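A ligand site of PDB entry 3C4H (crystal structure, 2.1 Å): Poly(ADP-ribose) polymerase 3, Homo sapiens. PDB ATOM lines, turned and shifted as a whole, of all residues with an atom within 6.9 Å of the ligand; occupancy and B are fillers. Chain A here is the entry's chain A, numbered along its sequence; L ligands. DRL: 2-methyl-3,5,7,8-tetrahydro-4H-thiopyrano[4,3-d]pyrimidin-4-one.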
ATOM      1  N   TRP A 208       9.516 -25.029   6.644  1.00  0.00           N
ATOM      2  CA  TRP A 208      10.956 -25.345   6.573  1.00  0.00           C
ATOM      3  C   TRP A 208      11.610 -24.987   5.264  1.00  0.00           C
ATOM      4  O   TRP A 208      11.008 -25.154   4.213  1.00  0.00           O
ATOM      5  CB  TRP A 208      11.172 -26.856   6.794  1.00  0.00           C
ATOM      6  CG  TRP A 208      10.707 -27.313   8.117  1.00  0.00           C
ATOM      7  CD1 TRP A 208       9.554 -27.984   8.412  1.00  0.00           C
ATOM      8  CD2 TRP A 208      11.371 -27.088   9.355  1.00  0.00           C
ATOM      9  NE1 TRP A 208       9.470 -28.220   9.769  1.00  0.00           N
ATOM     10  CE2 TRP A 208      10.575 -27.674  10.372  1.00  0.00           C
ATOM     11  CE3 TRP A 208      12.586 -26.472   9.716  1.00  0.00           C
ATOM     12  CZ2 TRP A 208      10.942 -27.645  11.723  1.00  0.00           C
ATOM     13  CZ3 TRP A 208      12.940 -26.444  11.063  1.00  0.00           C
ATOM     14  CH2 TRP A 208      12.119 -27.028  12.040  1.00  0.00           C
ATOM     15  N   HIS A 209      12.871 -24.550   5.339  1.00  0.00           N
ATOM     16  CA  HIS A 209      13.715 -24.426   4.168  1.00  0.00           C
ATOM     17  C   HIS A 209      15.115 -24.876   4.555  1.00  0.00           C
ATOM     18  O   HIS A 209      15.843 -24.186   5.299  1.00  0.00           O
ATOM     19  CB  HIS A 209      13.686 -23.005   3.594  1.00  0.00           C
ATOM     20  CG  HIS A 209      14.497 -22.855   2.334  1.00  0.00           C
ATOM     21  ND1 HIS A 209      13.946 -23.014   1.077  1.00  0.00           N
ATOM     22  CD2 HIS A 209      15.812 -22.587   2.142  1.00  0.00           C
ATOM     23  CE1 HIS A 209      14.895 -22.842   0.168  1.00  0.00           C
ATOM     24  NE2 HIS A 209      16.033 -22.585   0.784  1.00  0.00           N
ATOM     25  N   GLY A 210      15.477 -26.074   4.108  1.00  0.00           N
ATOM     26  CA  GLY A 210      16.792 -26.633   4.392  1.00  0.00           C
ATOM     27  C   GLY A 210      17.718 -26.089   3.351  1.00  0.00           C
ATOM     28  O   GLY A 210      17.292 -25.822   2.228  1.00  0.00           O
ATOM     29  N   THR A 211      18.993 -25.940   3.704  1.00  0.00           N
ATOM     30  CA  THR A 211      19.960 -25.299   2.816  1.00  0.00           C
ATOM     31  C   THR A 211      21.379 -25.786   3.104  1.00  0.00           C
ATOM     32  O   THR A 211      21.646 -26.280   4.198  1.00  0.00           O
ATOM     33  CB  THR A 211      19.890 -23.755   2.987  1.00  0.00           C
ATOM     34  OG1 THR A 211      20.741 -23.132   2.024  1.00  0.00           O
ATOM     35  CG2 THR A 211      20.341 -23.352   4.405  1.00  0.00           C
ATOM     36  N   ASN A 212      22.287 -25.666   2.151  1.00  0.00           N
ATOM     37  CA  ASN A 212      23.674 -25.933   2.510  1.00  0.00           C
ATOM     38  C   ASN A 212      24.304 -24.724   3.159  1.00  0.00           C
ATOM     39  O   ASN A 212      23.903 -23.589   2.908  1.00  0.00           O
ATOM     40  CB  ASN A 212      24.536 -26.484   1.377  1.00  0.00           C
ATOM     41  CG  ASN A 212      24.343 -25.770   0.070  1.00  0.00           C
ATOM     42  OD1 ASN A 212      23.557 -24.833  -0.027  1.00  0.00           O
ATOM     43  ND2 ASN A 212      25.040 -26.225  -0.947  1.00  0.00           N
ATOM     44  N   ARG A 233      10.756 -29.026  -9.331  1.00  0.00           N
ATOM     45  CA  ARG A 233       9.572 -29.800  -9.681  1.00  0.00           C
ATOM     46  C   ARG A 233       8.305 -28.952  -9.787  1.00  0.00           C
ATOM     47  O   ARG A 233       7.318 -29.374 -10.416  1.00  0.00           O
ATOM     48  CB  ARG A 233       9.357 -30.943  -8.693  1.00  0.00           C
ATOM     49  CG  ARG A 233      10.488 -31.968  -8.700  1.00  0.00           C
ATOM     50  CD  ARG A 233      10.226 -33.059  -7.693  1.00  0.00           C
ATOM     51  NE  ARG A 233       9.145 -33.927  -8.130  1.00  0.00           N
ATOM     52  CZ  ARG A 233       8.607 -34.909  -7.404  1.00  0.00           C
ATOM     53  NH1 ARG A 233       9.045 -35.180  -6.179  1.00  0.00           N
ATOM     54  NH2 ARG A 233       7.632 -35.632  -7.931  1.00  0.00           N
ATOM     55  N   TYR A 239      10.991 -22.599  -2.454  1.00  0.00           N
ATOM     56  CA  TYR A 239      10.514 -23.906  -2.025  1.00  0.00           C
ATOM     57  C   TYR A 239      10.543 -24.047  -0.506  1.00  0.00           C
ATOM     58  O   TYR A 239      11.555 -23.757   0.143  1.00  0.00           O
ATOM     59  CB  TYR A 239      11.404 -24.997  -2.633  1.00  0.00           C
ATOM     60  CG  TYR A 239      11.159 -25.225  -4.132  1.00  0.00           C
ATOM     61  CD1 TYR A 239      10.466 -26.358  -4.578  1.00  0.00           C
ATOM     62  CD2 TYR A 239      11.619 -24.322  -5.082  1.00  0.00           C
ATOM     63  CE1 TYR A 239      10.239 -26.583  -5.948  1.00  0.00           C
ATOM     64  CE2 TYR A 239      11.389 -24.534  -6.469  1.00  0.00           C
ATOM     65  CZ  TYR A 239      10.699 -25.664  -6.879  1.00  0.00           C
ATOM     66  OH  TYR A 239      10.446 -25.875  -8.216  1.00  0.00           O
ATOM     67  N   PHE A 240       9.400 -24.481   0.047  1.00  0.00           N
ATOM     68  CA  PHE A 240       9.279 -24.801   1.471  1.00  0.00           C
ATOM     69  C   PHE A 240       8.638 -26.167   1.660  1.00  0.00           C
ATOM     70  O   PHE A 240       8.037 -26.717   0.743  1.00  0.00           O
ATOM     71  CB  PHE A 240       8.438 -23.747   2.190  1.00  0.00           C
ATOM     72  CG  PHE A 240       8.944 -22.329   2.061  1.00  0.00           C
ATOM     73  CD1 PHE A 240       9.873 -21.825   2.965  1.00  0.00           C
ATOM     74  CD2 PHE A 240       8.475 -21.492   1.051  1.00  0.00           C
ATOM     75  CE1 PHE A 240      10.338 -20.528   2.876  1.00  0.00           C
ATOM     76  CE2 PHE A 240       8.932 -20.188   0.939  1.00  0.00           C
ATOM     77  CZ  PHE A 240       9.861 -19.702   1.869  1.00  0.00           C
ATOM     78  N   ALA A 241       8.769 -26.711   2.863  1.00  0.00           N
ATOM     79  CA  ALA A 241       8.152 -27.984   3.232  1.00  0.00           C
ATOM     80  C   ALA A 241       7.508 -27.851   4.602  1.00  0.00           C
ATOM     81  O   ALA A 241       8.002 -27.125   5.461  1.00  0.00           O
ATOM     82  CB  ALA A 241       9.190 -29.084   3.257  1.00  0.00           C
ATOM     83  N   GLU A 243       7.089 -30.706   6.144  1.00  0.00           N
ATOM     84  CA  GLU A 243       7.778 -31.836   6.750  1.00  0.00           C
ATOM     85  C   GLU A 243       9.283 -31.591   6.828  1.00  0.00           C
ATOM     86  O   GLU A 243       9.955 -31.433   5.812  1.00  0.00           O
ATOM     87  CB  GLU A 243       7.452 -33.156   6.019  1.00  0.00           C
ATOM     88  CG  GLU A 243       6.040 -33.654   6.311  1.00  0.00           C
ATOM     89  CD  GLU A 243       5.688 -34.960   5.634  1.00  0.00           C
ATOM     90  OE1 GLU A 243       6.397 -35.986   5.829  1.00  0.00           O
ATOM     91  OE2 GLU A 243       4.663 -34.966   4.909  1.00  0.00           O
ATOM     92  N   ASN A 244       9.785 -31.545   8.057  1.00  0.00           N
ATOM     93  CA  ASN A 244      11.203 -31.370   8.306  1.00  0.00           C
ATOM     94  C   ASN A 244      12.074 -32.350   7.525  1.00  0.00           C
ATOM     95  O   ASN A 244      13.072 -31.941   6.919  1.00  0.00           O
ATOM     96  CB  ASN A 244      11.502 -31.452   9.804  1.00  0.00           C
ATOM     97  CG  ASN A 244      12.954 -31.184  10.112  1.00  0.00           C
ATOM     98  OD1 ASN A 244      13.758 -32.113  10.173  1.00  0.00           O
ATOM     99  ND2 ASN A 244      13.313 -29.920  10.247  1.00  0.00           N
ATOM    100  N   LYS A 246      11.581 -33.790   4.656  1.00  0.00           N
ATOM    101  CA  LYS A 246      11.725 -33.325   3.266  1.00  0.00           C
ATOM    102  C   LYS A 246      12.798 -32.219   3.139  1.00  0.00           C
ATOM    103  O   LYS A 246      13.703 -32.305   2.290  1.00  0.00           O
ATOM    104  CB  LYS A 246      10.366 -32.833   2.740  1.00  0.00           C
ATOM    105  CG  LYS A 246      10.381 -32.158   1.376  1.00  0.00           C
ATOM    106  CD  LYS A 246      10.485 -33.145   0.224  1.00  0.00           C
ATOM    107  CE  LYS A 246       9.704 -32.598  -0.952  1.00  0.00           C
ATOM    108  NZ  LYS A 246      10.004 -33.290  -2.227  1.00  0.00           N
ATOM    109  N   SER A 247      12.711 -31.182   3.969  1.00  0.00           N
ATOM    110  CA  SER A 247      13.721 -30.112   3.955  1.00  0.00           C
ATOM    111  C   SER A 247      15.111 -30.560   4.396  1.00  0.00           C
ATOM    112  O   SER A 247      16.108 -30.040   3.904  1.00  0.00           O
ATOM    113  CB  SER A 247      13.267 -28.914   4.778  1.00  0.00           C
ATOM    114  OG  SER A 247      12.355 -28.108   4.041  1.00  0.00           O
ATOM    115  N   ALA A 248      15.169 -31.524   5.325  1.00  0.00           N
ATOM    116  CA  ALA A 248      16.449 -32.002   5.834  1.00  0.00           C
ATOM    117  C   ALA A 248      17.310 -32.654   4.749  1.00  0.00           C
ATOM    118  O   ALA A 248      18.544 -32.702   4.863  1.00  0.00           O
ATOM    119  CB  ALA A 248      16.246 -32.971   7.021  1.00  0.00           C
ATOM    120  N   GLY A 249      16.660 -33.149   3.695  1.00  0.00           N
ATOM    121  CA  GLY A 249      17.368 -33.718   2.532  1.00  0.00           C
ATOM    122  C   GLY A 249      18.206 -32.688   1.790  1.00  0.00           C
ATOM    123  O   GLY A 249      19.159 -33.047   1.089  1.00  0.00           O
ATOM    124  N   TYR A 250      17.870 -31.414   1.952  1.00  0.00           N
ATOM    125  CA  TYR A 250      18.591 -30.324   1.279  1.00  0.00           C
ATOM    126  C   TYR A 250      19.615 -29.662   2.175  1.00  0.00           C
ATOM    127  O   TYR A 250      20.261 -28.697   1.787  1.00  0.00           O
ATOM    128  CB  TYR A 250      17.599 -29.312   0.693  1.00  0.00           C
ATOM    129  CG  TYR A 250      16.676 -29.937  -0.316  1.00  0.00           C
ATOM    130  CD1 TYR A 250      17.033 -30.004  -1.663  1.00  0.00           C
ATOM    131  CD2 TYR A 250      15.466 -30.504   0.085  1.00  0.00           C
ATOM    132  CE1 TYR A 250      16.194 -30.603  -2.592  1.00  0.00           C
ATOM    133  CE2 TYR A 250      14.616 -31.101  -0.835  1.00  0.00           C
ATOM    134  CZ  TYR A 250      14.984 -31.154  -2.173  1.00  0.00           C
ATOM    135  OH  TYR A 250      14.153 -31.759  -3.080  1.00  0.00           O
ATOM    136  N   VAL A 251      19.773 -30.203   3.386  1.00  0.00           N
ATOM    137  CA  VAL A 251      20.746 -29.710   4.343  1.00  0.00           C
ATOM    138  C   VAL A 251      22.063 -30.381   4.066  1.00  0.00           C
ATOM    139  O   VAL A 251      22.275 -31.553   4.404  1.00  0.00           O
ATOM    140  CB  VAL A 251      20.292 -29.925   5.826  1.00  0.00           C
ATOM    141  CG1 VAL A 251      21.382 -29.510   6.807  1.00  0.00           C
ATOM    142  CG2 VAL A 251      19.021 -29.177   6.103  1.00  0.00           C
ATOM    143  N   MET A 264      18.948 -24.942   9.136  1.00  0.00           N
ATOM    144  CA  MET A 264      17.644 -24.938   8.490  1.00  0.00           C
ATOM    145  C   MET A 264      16.928 -23.675   8.862  1.00  0.00           C
ATOM    146  O   MET A 264      17.018 -23.244  10.008  1.00  0.00           O
ATOM    147  CB  MET A 264      16.830 -26.175   8.907  1.00  0.00           C
ATOM    148  CG  MET A 264      17.542 -27.515   8.682  1.00  0.00           C
ATOM    149  SD  MET A 264      16.548 -29.002   8.910  1.00  0.00           S
ATOM    150  CE  MET A 264      15.246 -28.694   7.696  1.00  0.00           C
ATOM    151  N   SER A 338       4.737 -32.828   0.560  1.00  0.00           N
ATOM    152  CA  SER A 338       4.364 -31.544  -0.070  1.00  0.00           C
ATOM    153  C   SER A 338       5.552 -30.614  -0.281  1.00  0.00           C
ATOM    154  O   SER A 338       6.503 -30.609   0.512  1.00  0.00           O
ATOM    155  CB  SER A 338       3.276 -30.820   0.755  1.00  0.00           C
ATOM    156  OG  SER A 338       2.112 -31.617   0.906  1.00  0.00           O
ATOM    157  N   GLU A 339       5.483 -29.827  -1.364  1.00  0.00           N
ATOM    158  CA  GLU A 339       6.378 -28.703  -1.614  1.00  0.00           C
ATOM    159  C   GLU A 339       5.523 -27.443  -1.733  1.00  0.00           C
ATOM    160  O   GLU A 339       4.652 -27.357  -2.611  1.00  0.00           O
ATOM    161  CB  GLU A 339       7.192 -28.931  -2.884  1.00  0.00           C
ATOM    162  CG  GLU A 339       7.973 -30.252  -2.869  1.00  0.00           C
ATOM    163  CD  GLU A 339       8.971 -30.407  -3.988  1.00  0.00           C
ATOM    164  OE1 GLU A 339       9.163 -29.465  -4.787  1.00  0.00           O
ATOM    165  OE2 GLU A 339       9.585 -31.499  -4.061  1.00  0.00           O
ATOM    166  N   TYR A 340       5.765 -26.470  -0.845  1.00  0.00           N
ATOM    167  CA  TYR A 340       5.003 -25.226  -0.786  1.00  0.00           C
ATOM    168  C   TYR A 340       5.744 -24.140  -1.544  1.00  0.00           C
ATOM    169  O   TYR A 340       6.900 -23.849  -1.223  1.00  0.00           O
ATOM    170  CB  TYR A 340       4.845 -24.766   0.659  1.00  0.00           C
ATOM    171  CG  TYR A 340       3.853 -25.556   1.478  1.00  0.00           C
ATOM    172  CD1 TYR A 340       2.657 -24.978   1.886  1.00  0.00           C
ATOM    173  CD2 TYR A 340       4.140 -26.864   1.894  1.00  0.00           C
ATOM    174  CE1 TYR A 340       1.742 -25.697   2.656  1.00  0.00           C
ATOM    175  CE2 TYR A 340       3.254 -27.593   2.646  1.00  0.00           C
ATOM    176  CZ  TYR A 340       2.055 -27.002   3.036  1.00  0.00           C
ATOM    177  OH  TYR A 340       1.166 -27.702   3.788  1.00  0.00           O
ATOM    178  N   LEU A 341       5.074 -23.537  -2.520  1.00  0.00           N
ATOM    179  CA  LEU A 341       5.698 -22.569  -3.417  1.00  0.00           C
ATOM    180  C   LEU A 341       5.058 -21.193  -3.402  1.00  0.00           C
ATOM    181  O   LEU A 341       3.848 -21.050  -3.492  1.00  0.00           O
ATOM    182  CB  LEU A 341       5.673 -23.103  -4.856  1.00  0.00           C
ATOM    183  CG  LEU A 341       6.724 -24.121  -5.309  1.00  0.00           C
ATOM    184  CD1 LEU A 341       8.084 -23.462  -5.481  1.00  0.00           C
ATOM    185  CD2 LEU A 341       6.809 -25.346  -4.357  1.00  0.00           C
HETATM  186  C1A DRL L   1      16.910 -25.808  -1.126  1.00  0.00           C
HETATM  187  C1I DRL L   1      15.582 -26.481  -0.726  1.00  0.00           C
HETATM  188  N1G DRL L   1      14.778 -27.018  -1.640  1.00  0.00           N
HETATM  189  C1J DRL L   1      13.609 -27.610  -1.339  1.00  0.00           C
HETATM  190  C1D DRL L   1      12.881 -28.169  -2.577  1.00  0.00           C
HETATM  191  C1C DRL L   1      11.814 -29.208  -2.230  1.00  0.00           C
HETATM  192  S1H DRL L   1      10.685 -28.500  -0.998  1.00  0.00           S
HETATM  193  C1E DRL L   1      11.864 -28.379   0.402  1.00  0.00           C
HETATM  194  C1K DRL L   1      13.189 -27.709  -0.011  1.00  0.00           C
HETATM  195  C1L DRL L   1      14.026 -27.147   0.957  1.00  0.00           C
HETATM  196  O1B DRL L   1      13.734 -27.173   2.150  1.00  0.00           O
HETATM  197  N1F DRL L   1      15.224 -26.548   0.611  1.00  0.00           N
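The backbone carbonyl oxygen of Phe 240 lies close to a sulfur (S1H) of the ligand (3.6 Å). Trp 208 touches the ligand. His 209 touches the ligand. CB of Tyr 239 touches C1D of the ligand, 3.5 Å away. Ala 241 touches the ligand (CB to C1E, 3.97 Å). Tyr 250 touches the ligand. CD of Glu 339 touches C1C of the ligand (3.6 Å). Nine residues have an atom within 4 Å of the ligand: Trp 208, His 209, Gly 210, Tyr 239, Phe 240, Ala 241, Ser 247, Tyr 250 and Glu 339. Along chain A the residues within 4 Å of the ligand span positions 208 to 339. The nearest printed residue that does not touch the ligand is Lys 246 (4.2 Å).
O of Phe 240 is in hydrogen-bond range of N of Tyr 340 (2.8 Å). The side-chain hydroxyl (OH) of Tyr 239 sits at hydrogen-bond distance from the backbone NH (N) of Arg 233 (3.4 Å). O of Tyr 239 lies within hydrogen-bond range of ND1 of His 209, 2.7 Å away. The side-chain hydroxyl of Ser 247 lies close to the backbone carbonyl oxygen of Trp 208, 3.3 Å away. The backbone NH (N) of Trp 208 sits at hydrogen-bond distance from the backbone carbonyl oxygen (O) of Ala 241 (2.8 Å). OE2 of Glu 339 lies within salt-bridge range of NZ of Lys 246, 2.6 Å away.
N1F of the ligand is in hydrogen-bond range of O of Gly 210 (2.7 Å). The backbone NH (N) of Gly 210 sits at hydrogen-bond distance from an oxygen (O1B) of the ligand (2.8 Å). An oxygen (O1B) of the ligand lies within hydrogen-bond range of the side-chain hydroxyl of Ser 247, at 2.5 Å.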
